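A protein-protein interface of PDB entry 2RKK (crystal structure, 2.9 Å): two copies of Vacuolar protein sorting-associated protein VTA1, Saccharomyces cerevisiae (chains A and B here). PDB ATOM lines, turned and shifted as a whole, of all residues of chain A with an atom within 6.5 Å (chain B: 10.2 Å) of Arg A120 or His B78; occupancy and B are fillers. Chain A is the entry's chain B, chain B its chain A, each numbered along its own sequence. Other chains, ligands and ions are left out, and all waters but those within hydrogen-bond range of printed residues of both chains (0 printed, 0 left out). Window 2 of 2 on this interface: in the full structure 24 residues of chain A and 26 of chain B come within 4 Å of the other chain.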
ATOM      1  N   ASP A  15      15.241 -24.830   1.041  1.00  0.00           N
ATOM      2  CA  ASP A  15      16.678 -24.614   1.099  1.00  0.00           C
ATOM      3  C   ASP A  15      17.122 -23.662   0.000  1.00  0.00           C
ATOM      4  O   ASP A  15      18.065 -22.892   0.178  1.00  0.00           O
ATOM      5  CB  ASP A  15      17.432 -25.936   0.953  1.00  0.00           C
ATOM      6  CG  ASP A  15      17.798 -26.542   2.283  1.00  0.00           C
ATOM      7  OD1 ASP A  15      16.889 -26.883   3.074  1.00  0.00           O
ATOM      8  OD2 ASP A  15      19.011 -26.674   2.546  1.00  0.00           O
ATOM      9  N   VAL A  19      18.953 -19.669   0.034  1.00  0.00           N
ATOM     10  CA  VAL A  19      20.147 -19.319  -0.744  1.00  0.00           C
ATOM     11  C   VAL A  19      19.876 -18.097  -1.620  1.00  0.00           C
ATOM     12  O   VAL A  19      20.708 -17.197  -1.732  1.00  0.00           O
ATOM     13  CB  VAL A  19      20.587 -20.480  -1.682  1.00  0.00           C
ATOM     14  CG1 VAL A  19      21.986 -20.222  -2.236  1.00  0.00           C
ATOM     15  CG2 VAL A  19      20.553 -21.786  -0.941  1.00  0.00           C
ATOM     16  N   LYS A 105      29.354 -32.315  -9.190  1.00  0.00           N
ATOM     17  CA  LYS A 105      29.224 -33.459  -8.300  1.00  0.00           C
ATOM     18  C   LYS A 105      29.839 -34.739  -8.867  1.00  0.00           C
ATOM     19  O   LYS A 105      30.330 -35.572  -8.108  1.00  0.00           O
ATOM     20  CB  LYS A 105      27.752 -33.676  -7.936  1.00  0.00           C
ATOM     21  CG  LYS A 105      27.180 -32.541  -7.094  1.00  0.00           C
ATOM     22  CD  LYS A 105      28.032 -32.300  -5.865  1.00  0.00           C
ATOM     23  CE  LYS A 105      27.804 -30.924  -5.290  1.00  0.00           C
ATOM     24  NZ  LYS A 105      28.544 -30.782  -4.008  1.00  0.00           N
ATOM     25  N   ASP A 115      31.796 -36.848   1.582  1.00  0.00           N
ATOM     26  CA  ASP A 115      31.052 -36.546   2.800  1.00  0.00           C
ATOM     27  C   ASP A 115      29.535 -36.489   2.605  1.00  0.00           C
ATOM     28  O   ASP A 115      29.014 -36.823   1.539  1.00  0.00           O
ATOM     29  CB  ASP A 115      31.544 -35.214   3.385  1.00  0.00           C
ATOM     30  CG  ASP A 115      31.326 -34.030   2.436  1.00  0.00           C
ATOM     31  OD1 ASP A 115      31.744 -34.108   1.254  1.00  0.00           O
ATOM     32  OD2 ASP A 115      30.747 -33.018   2.886  1.00  0.00           O
ATOM     33  N   VAL A 116      28.838 -36.065   3.654  1.00  0.00           N
ATOM     34  CA  VAL A 116      27.387 -35.944   3.613  1.00  0.00           C
ATOM     35  C   VAL A 116      26.967 -35.067   2.438  1.00  0.00           C
ATOM     36  O   VAL A 116      26.019 -35.385   1.714  1.00  0.00           O
ATOM     37  CB  VAL A 116      26.836 -35.289   4.897  1.00  0.00           C
ATOM     38  CG1 VAL A 116      25.318 -35.209   4.836  1.00  0.00           C
ATOM     39  CG2 VAL A 116      27.289 -36.068   6.111  1.00  0.00           C
ATOM     40  N   MET A 117      27.676 -33.956   2.259  1.00  0.00           N
ATOM     41  CA  MET A 117      27.384 -33.014   1.185  1.00  0.00           C
ATOM     42  C   MET A 117      27.234 -33.712  -0.146  1.00  0.00           C
ATOM     43  O   MET A 117      26.246 -33.519  -0.848  1.00  0.00           O
ATOM     44  CB  MET A 117      28.487 -31.960   1.078  1.00  0.00           C
ATOM     45  CG  MET A 117      28.116 -30.746   0.225  1.00  0.00           C
ATOM     46  SD  MET A 117      26.501 -29.958   0.661  1.00  0.00           S
ATOM     47  CE  MET A 117      26.465 -30.028   2.558  1.00  0.00           C
ATOM     48  N   LEU A 118      28.218 -34.526  -0.498  1.00  0.00           N
ATOM     49  CA  LEU A 118      28.148 -35.241  -1.756  1.00  0.00           C
ATOM     50  C   LEU A 118      26.841 -36.030  -1.825  1.00  0.00           C
ATOM     51  O   LEU A 118      26.234 -36.148  -2.890  1.00  0.00           O
ATOM     52  CB  LEU A 118      29.343 -36.178  -1.892  1.00  0.00           C
ATOM     53  CG  LEU A 118      29.328 -36.890  -3.239  1.00  0.00           C
ATOM     54  CD1 LEU A 118      29.289 -35.860  -4.367  1.00  0.00           C
ATOM     55  CD2 LEU A 118      30.546 -37.780  -3.345  1.00  0.00           C
ATOM     56  N   LYS A 119      26.414 -36.562  -0.680  1.00  0.00           N
ATOM     57  CA  LYS A 119      25.175 -37.339  -0.585  1.00  0.00           C
ATOM     58  C   LYS A 119      23.965 -36.447  -0.864  1.00  0.00           C
ATOM     59  O   LYS A 119      23.171 -36.724  -1.767  1.00  0.00           O
ATOM     60  CB  LYS A 119      25.055 -37.963   0.814  1.00  0.00           C
ATOM     61  CG  LYS A 119      25.046 -39.493   0.839  1.00  0.00           C
ATOM     62  CD  LYS A 119      25.192 -40.057   2.268  1.00  0.00           C
ATOM     63  CE  LYS A 119      26.625 -39.898   2.848  1.00  0.00           C
ATOM     64  NZ  LYS A 119      27.669 -40.829   2.278  1.00  0.00           N
ATOM     65  N   ARG A 120      23.833 -35.380  -0.076  1.00  0.00           N
ATOM     66  CA  ARG A 120      22.736 -34.422  -0.226  1.00  0.00           C
ATOM     67  C   ARG A 120      22.669 -33.911  -1.652  1.00  0.00           C
ATOM     68  O   ARG A 120      21.586 -33.751  -2.219  1.00  0.00           O
ATOM     69  CB  ARG A 120      22.932 -33.215   0.690  1.00  0.00           C
ATOM     70  CG  ARG A 120      22.515 -33.413   2.127  1.00  0.00           C
ATOM     71  CD  ARG A 120      22.831 -32.156   2.921  1.00  0.00           C
ATOM     72  NE  ARG A 120      22.299 -30.942   2.299  1.00  0.00           N
ATOM     73  CZ  ARG A 120      22.627 -29.710   2.688  1.00  0.00           C
ATOM     74  NH1 ARG A 120      23.483 -29.561   3.692  1.00  0.00           N
ATOM     75  NH2 ARG A 120      22.107 -28.635   2.086  1.00  0.00           N
ATOM     76  N   SER A 121      23.845 -33.642  -2.211  1.00  0.00           N
ATOM     77  CA  SER A 121      23.980 -33.128  -3.566  1.00  0.00           C
ATOM     78  C   SER A 121      23.414 -34.097  -4.585  1.00  0.00           C
ATOM     79  O   SER A 121      22.678 -33.693  -5.486  1.00  0.00           O
ATOM     80  CB  SER A 121      25.456 -32.853  -3.883  1.00  0.00           C
ATOM     81  OG  SER A 121      25.959 -31.759  -3.128  1.00  0.00           O
ATOM     82  N   LEU A 122      23.755 -35.375  -4.445  1.00  0.00           N
ATOM     83  CA  LEU A 122      23.273 -36.402  -5.373  1.00  0.00           C
ATOM     84  C   LEU A 122      21.750 -36.507  -5.352  1.00  0.00           C
ATOM     85  O   LEU A 122      21.116 -36.713  -6.390  1.00  0.00           O
ATOM     86  CB  LEU A 122      23.903 -37.760  -5.038  1.00  0.00           C
ATOM     87  CG  LEU A 122      25.400 -37.912  -5.352  1.00  0.00           C
ATOM     88  CD1 LEU A 122      25.826 -39.358  -5.121  1.00  0.00           C
ATOM     89  CD2 LEU A 122      25.670 -37.514  -6.783  1.00  0.00           C
ATOM     90  N   TRP A 123      21.171 -36.356  -4.167  1.00  0.00           N
ATOM     91  CA  TRP A 123      19.727 -36.422  -4.022  1.00  0.00           C
ATOM     92  C   TRP A 123      19.084 -35.202  -4.643  1.00  0.00           C
ATOM     93  O   TRP A 123      17.999 -35.271  -5.213  1.00  0.00           O
ATOM     94  CB  TRP A 123      19.350 -36.493  -2.551  1.00  0.00           C
ATOM     95  CG  TRP A 123      19.310 -37.867  -2.045  1.00  0.00           C
ATOM     96  CD1 TRP A 123      20.189 -38.445  -1.195  1.00  0.00           C
ATOM     97  CD2 TRP A 123      18.312 -38.848  -2.324  1.00  0.00           C
ATOM     98  NE1 TRP A 123      19.803 -39.731  -0.911  1.00  0.00           N
ATOM     99  CE2 TRP A 123      18.649 -40.007  -1.595  1.00  0.00           C
ATOM    100  CE3 TRP A 123      17.160 -38.861  -3.122  1.00  0.00           C
ATOM    101  CZ2 TRP A 123      17.877 -41.174  -1.628  1.00  0.00           C
ATOM    102  CZ3 TRP A 123      16.389 -40.022  -3.160  1.00  0.00           C
ATOM    103  CH2 TRP A 123      16.755 -41.164  -2.414  1.00  0.00           C
ATOM    104  N   CYS A 124      19.770 -34.080  -4.506  1.00  0.00           N
ATOM    105  CA  CYS A 124      19.298 -32.838  -5.058  1.00  0.00           C
ATOM    106  C   CYS A 124      19.215 -33.032  -6.570  1.00  0.00           C
ATOM    107  O   CYS A 124      18.192 -32.731  -7.185  1.00  0.00           O
ATOM    108  CB  CYS A 124      20.279 -31.721  -4.715  1.00  0.00           C
ATOM    109  SG  CYS A 124      19.699 -30.081  -5.072  1.00  0.00           S
ATOM    110  N   CYS A 125      20.274 -33.569  -7.164  1.00  0.00           N
ATOM    111  CA  CYS A 125      20.283 -33.786  -8.601  1.00  0.00           C
ATOM    112  C   CYS A 125      19.118 -34.692  -8.993  1.00  0.00           C
ATOM    113  O   CYS A 125      18.418 -34.421  -9.971  1.00  0.00           O
ATOM    114  CB  CYS A 125      21.618 -34.387  -9.041  1.00  0.00           C
ATOM    115  SG  CYS A 125      23.017 -33.329  -8.618  1.00  0.00           S
ATOM    116  N   LEU A 159      24.976 -43.311  -5.030  1.00  0.00           N
ATOM    117  CA  LEU A 159      24.499 -43.255  -3.652  1.00  0.00           C
ATOM    118  C   LEU A 159      24.678 -44.660  -3.042  1.00  0.00           C
ATOM    119  O   LEU A 159      25.129 -44.801  -1.895  1.00  0.00           O
ATOM    120  CB  LEU A 159      23.027 -42.822  -3.595  1.00  0.00           C
ATOM    121  CG  LEU A 159      22.757 -41.320  -3.619  1.00  0.00           C
ATOM    122  CD1 LEU A 159      21.253 -41.066  -3.626  1.00  0.00           C
ATOM    123  CD2 LEU A 159      23.400 -40.664  -2.423  1.00  0.00           C
ATOM    124  N   ILE B  23      21.428 -15.260  -6.531  1.00  0.00           N
ATOM    125  CA  ILE B  23      22.811 -15.305  -6.937  1.00  0.00           C
ATOM    126  C   ILE B  23      23.091 -14.254  -8.014  1.00  0.00           C
ATOM    127  O   ILE B  23      24.124 -13.564  -7.979  1.00  0.00           O
ATOM    128  CB  ILE B  23      23.207 -16.693  -7.454  1.00  0.00           C
ATOM    129  CG1 ILE B  23      23.279 -17.683  -6.275  1.00  0.00           C
ATOM    130  CG2 ILE B  23      24.564 -16.624  -8.143  1.00  0.00           C
ATOM    131  CD1 ILE B  23      23.735 -19.091  -6.667  1.00  0.00           C
ATOM    132  N   LYS B  61      26.319 -13.818   1.351  1.00  0.00           N
ATOM    133  CA  LYS B  61      27.375 -14.832   1.312  1.00  0.00           C
ATOM    134  C   LYS B  61      27.450 -15.579   2.624  1.00  0.00           C
ATOM    135  O   LYS B  61      27.672 -16.788   2.648  1.00  0.00           O
ATOM    136  CB  LYS B  61      28.735 -14.194   1.014  1.00  0.00           C
ATOM    137  CG  LYS B  61      29.842 -15.223   0.778  1.00  0.00           C
ATOM    138  CD  LYS B  61      31.160 -14.572   0.405  1.00  0.00           C
ATOM    139  CE  LYS B  61      32.260 -15.608   0.206  1.00  0.00           C
ATOM    140  NZ  LYS B  61      33.514 -14.960  -0.272  1.00  0.00           N
ATOM    141  N   LYS B  62      27.276 -14.840   3.713  1.00  0.00           N
ATOM    142  CA  LYS B  62      27.301 -15.441   5.026  1.00  0.00           C
ATOM    143  C   LYS B  62      26.259 -16.538   5.123  1.00  0.00           C
ATOM    144  O   LYS B  62      26.542 -17.625   5.611  1.00  0.00           O
ATOM    145  CB  LYS B  62      27.025 -14.409   6.110  1.00  0.00           C
ATOM    146  CG  LYS B  62      26.923 -15.018   7.496  1.00  0.00           C
ATOM    147  CD  LYS B  62      26.781 -13.941   8.550  1.00  0.00           C
ATOM    148  CE  LYS B  62      26.695 -14.515   9.956  1.00  0.00           C
ATOM    149  NZ  LYS B  62      26.598 -13.403  10.943  1.00  0.00           N
ATOM    150  N   GLU B  63      25.052 -16.269   4.649  1.00  0.00           N
ATOM    151  CA  GLU B  63      23.995 -17.257   4.736  1.00  0.00           C
ATOM    152  C   GLU B  63      24.113 -18.437   3.763  1.00  0.00           C
ATOM    153  O   GLU B  63      23.197 -19.254   3.671  1.00  0.00           O
ATOM    154  CB  GLU B  63      22.660 -16.536   4.583  1.00  0.00           C
ATOM    155  CG  GLU B  63      21.635 -16.932   5.619  1.00  0.00           C
ATOM    156  CD  GLU B  63      20.825 -18.129   5.183  1.00  0.00           C
ATOM    157  OE1 GLU B  63      19.995 -17.959   4.254  1.00  0.00           O
ATOM    158  OE2 GLU B  63      21.028 -19.245   5.747  1.00  0.00           O
ATOM    159  N   ILE B  64      25.248 -18.552   3.074  1.00  0.00           N
ATOM    160  CA  ILE B  64      25.447 -19.644   2.112  1.00  0.00           C
ATOM    161  C   ILE B  64      26.851 -20.291   2.151  1.00  0.00           C
ATOM    162  O   ILE B  64      27.073 -21.356   1.568  1.00  0.00           O
ATOM    163  CB  ILE B  64      25.127 -19.133   0.679  1.00  0.00           C
ATOM    164  CG1 ILE B  64      23.627 -18.813   0.585  1.00  0.00           C
ATOM    165  CG2 ILE B  64      25.475 -20.185  -0.373  1.00  0.00           C
ATOM    166  CD1 ILE B  64      23.296 -17.365   0.290  1.00  0.00           C
ATOM    167  N   GLY B  65      27.789 -19.646   2.847  1.00  0.00           N
ATOM    168  CA  GLY B  65      29.143 -20.165   2.942  1.00  0.00           C
ATOM    169  C   GLY B  65      29.273 -21.352   3.874  1.00  0.00           C
ATOM    170  O   GLY B  65      30.251 -22.104   3.808  1.00  0.00           O
ATOM    171  N   LEU B  77      20.940 -25.326   0.298  1.00  0.00           N
ATOM    172  CA  LEU B  77      21.599 -24.222   1.003  1.00  0.00           C
ATOM    173  C   LEU B  77      23.113 -24.401   0.941  1.00  0.00           C
ATOM    174  O   LEU B  77      23.829 -23.559   0.400  1.00  0.00           O
ATOM    175  CB  LEU B  77      21.132 -24.175   2.466  1.00  0.00           C
ATOM    176  CG  LEU B  77      21.764 -23.135   3.401  1.00  0.00           C
ATOM    177  CD1 LEU B  77      21.370 -21.738   2.972  1.00  0.00           C
ATOM    178  CD2 LEU B  77      21.307 -23.397   4.835  1.00  0.00           C
ATOM    179  N   HIS B  78      23.591 -25.508   1.498  1.00  0.00           N
ATOM    180  CA  HIS B  78      25.017 -25.804   1.501  1.00  0.00           C
ATOM    181  C   HIS B  78      25.416 -26.439   0.156  1.00  0.00           C
ATOM    182  O   HIS B  78      26.591 -26.689  -0.095  1.00  0.00           O
ATOM    183  CB  HIS B  78      25.352 -26.787   2.641  1.00  0.00           C
ATOM    184  CG  HIS B  78      24.902 -26.346   4.006  1.00  0.00           C
ATOM    185  ND1 HIS B  78      25.755 -25.773   4.928  1.00  0.00           N
ATOM    186  CD2 HIS B  78      23.694 -26.428   4.618  1.00  0.00           C
ATOM    187  CE1 HIS B  78      25.093 -25.524   6.045  1.00  0.00           C
ATOM    188  NE2 HIS B  78      23.841 -25.912   5.883  1.00  0.00           N
ATOM    189  N   VAL B  79      24.445 -26.689  -0.714  1.00  0.00           N
ATOM    190  CA  VAL B  79      24.750 -27.336  -1.985  1.00  0.00           C
ATOM    191  C   VAL B  79      25.239 -26.389  -3.074  1.00  0.00           C
ATOM    192  O   VAL B  79      26.075 -26.755  -3.904  1.00  0.00           O
ATOM    193  CB  VAL B  79      23.518 -28.091  -2.505  1.00  0.00           C
ATOM    194  CG1 VAL B  79      23.919 -29.057  -3.588  1.00  0.00           C
ATOM    195  CG2 VAL B  79      22.840 -28.802  -1.366  1.00  0.00           C
ATOM    196  N   MET B  80      24.738 -25.158  -3.041  1.00  0.00           N
ATOM    197  CA  MET B  80      25.074 -24.142  -4.036  1.00  0.00           C
ATOM    198  C   MET B  80      26.262 -23.234  -3.751  1.00  0.00           C
ATOM    199  O   MET B  80      26.769 -22.589  -4.660  1.00  0.00           O
ATOM    200  CB  MET B  80      23.842 -23.283  -4.301  1.00  0.00           C
ATOM    201  CG  MET B  80      22.808 -24.009  -5.123  1.00  0.00           C
ATOM    202  SD  MET B  80      23.648 -24.856  -6.512  1.00  0.00           S
ATOM    203  CE  MET B  80      23.125 -26.556  -6.210  1.00  0.00           C
ATOM    204  N   ASN B  81      26.695 -23.188  -2.495  1.00  0.00           N
ATOM    205  CA  ASN B  81      27.813 -22.345  -2.074  1.00  0.00           C
ATOM    206  C   ASN B  81      28.888 -22.143  -3.139  1.00  0.00           C
ATOM    207  O   ASN B  81      29.417 -21.045  -3.296  1.00  0.00           O
ATOM    208  CB  ASN B  81      28.468 -22.935  -0.824  1.00  0.00           C
ATOM    209  CG  ASN B  81      29.172 -24.256  -1.107  1.00  0.00           C
ATOM    210  OD1 ASN B  81      28.524 -25.260  -1.392  1.00  0.00           O
ATOM    211  ND2 ASN B  81      30.504 -24.257  -1.050  1.00  0.00           N
ATOM    212  N   THR B  82      29.208 -23.214  -3.854  1.00  0.00           N
ATOM    213  CA  THR B  82      30.231 -23.194  -4.890  1.00  0.00           C
ATOM    214  C   THR B  82      30.084 -22.071  -5.905  1.00  0.00           C
ATOM    215  O   THR B  82      31.063 -21.649  -6.516  1.00  0.00           O
ATOM    216  CB  THR B  82      30.244 -24.531  -5.629  1.00  0.00           C
ATOM    217  OG1 THR B  82      29.037 -25.250  -5.325  1.00  0.00           O
ATOM    218  CG2 THR B  82      31.441 -25.346  -5.213  1.00  0.00           C
ATOM    219  N   LEU B  83      28.855 -21.592  -6.075  1.00  0.00           N
ATOM    220  CA  LEU B  83      28.552 -20.508  -7.006  1.00  0.00           C
ATOM    221  C   LEU B  83      28.892 -19.163  -6.394  1.00  0.00           C
ATOM    222  O   LEU B  83      28.806 -18.140  -7.058  1.00  0.00           O
ATOM    223  CB  LEU B  83      27.067 -20.517  -7.361  1.00  0.00           C
ATOM    224  CG  LEU B  83      26.620 -21.560  -8.363  1.00  0.00           C
ATOM    225  CD1 LEU B  83      25.121 -21.472  -8.557  1.00  0.00           C
ATOM    226  CD2 LEU B  83      27.353 -21.319  -9.669  1.00  0.00           C
ATOM    227  N   ILE B  84      29.252 -19.172  -5.118  1.00  0.00           N
ATOM    228  CA  ILE B  84      29.604 -17.948  -4.426  1.00  0.00           C
ATOM    229  C   ILE B  84      31.065 -17.998  -4.014  1.00  0.00           C
ATOM    230  O   ILE B  84      31.703 -16.963  -3.802  1.00  0.00           O
ATOM    231  CB  ILE B  84      28.759 -17.747  -3.167  1.00  0.00           C
ATOM    232  CG1 ILE B  84      27.279 -17.867  -3.511  1.00  0.00           C
ATOM    233  CG2 ILE B  84      29.019 -16.366  -2.581  1.00  0.00           C
ATOM    234  CD1 ILE B  84      26.384 -17.750  -2.292  1.00  0.00           C
ATOM    235  N   HIS B  85      31.595 -19.208  -3.901  1.00  0.00           N
ATOM    236  CA  HIS B  85      32.986 -19.377  -3.525  1.00  0.00           C
ATOM    237  C   HIS B  85      33.890 -19.625  -4.730  1.00  0.00           C
ATOM    238  O   HIS B  85      35.049 -19.221  -4.711  1.00  0.00           O
ATOM    239  CB  HIS B  85      33.129 -20.506  -2.490  1.00  0.00           C
ATOM    240  CG  HIS B  85      32.488 -20.190  -1.173  1.00  0.00           C
ATOM    241  ND1 HIS B  85      32.773 -19.042  -0.464  1.00  0.00           N
ATOM    242  CD2 HIS B  85      31.550 -20.851  -0.453  1.00  0.00           C
ATOM    243  CE1 HIS B  85      32.035 -19.006   0.632  1.00  0.00           C
ATOM    244  NE2 HIS B  85      31.284 -20.093   0.662  1.00  0.00           N
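Of the 15 printed residues of chain A, 5 touch a printed residue of chain B. Hydrophobic or aromatic side chains of chain A that line the printed part of chain B: Val A19 and Met A117. Hydrophobic or aromatic side chains of chain B that line the printed part of chain A: Ile B64, Leu B77, His B78 and Val B79. Among the printed residues, 8 pairs touch across the chains. Among the printed residues, no Asp or Glu carboxylate lies within 4 Å of a Lys or Arg side-chain nitrogen of the other chain.
Among the printed residues, pairs that only touch across the chains: Arg A120 with His B78 (3.3 Å), Val A19 with Leu B77 (3.3 Å), Val A19 with Ile B64 (3.3 Å), Ser A121 with Val B79 (3.4 Å), Arg A120 with Val B79 (3.5 Å) and Arg A120 with Leu B77 (3.9 Å).
Printed residues of chain B within 4 Å of Asp A15: Leu B77. Val A116 touches none of the printed residues of chain B. Of chain B, only His B78 comes within 4 Å of Met A117. Arg A120 touches just these residues of chain B: Leu B77, His B78 and Val B79. Of the printed residues of chain B, Ser A121 touches Val B79 (3.4 Å). No residue of chain B comes within 4 Å of Cys A124. Printed residues of chain A within 4 Å of Ile B64: Val A19. Of chain A, only Met A117 and Arg A120 come within 4 Å of His B78. Of the printed residues of chain A, Val B79 touches Arg A120 and Ser A121. The nearest printed residue of chain A that does not touch Val B79 is Met A117 (4.1 Å).
The side-chain amide oxygen (OD1) of Asn B81 sits close to the backbone carbonyl oxygen (O) of His B78, at 2.7 Å. OD2 of Asp A15 is in salt-bridge range of NH2 of Arg A120, at 3.7 Å. OG of Ser A121 lies within hydrogen-bond range of NZ of Lys A105 (2.9 Å). The backbone NH (N) of Met A117 sits close to the side-chain carboxylate (OD2) of Asp A115 (3.3 Å). The side-chain hydroxyl (OG) of Ser A121 sits at hydrogen-bond distance from the backbone carbonyl oxygen (O) of Met A117 (2.9 Å). The backbone carbonyl oxygen of Ser A121 is in hydrogen-bond range of the side-chain sulfur of Cys A125, at 3.2 Å.
N of Leu B77 is in hydrogen-bond range of OD2 of Asp A15. The side-chain sulfur of Met A117 sits close to the backbone carbonyl oxygen of His B78 (3.4 Å).
No position is printed for both chains.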
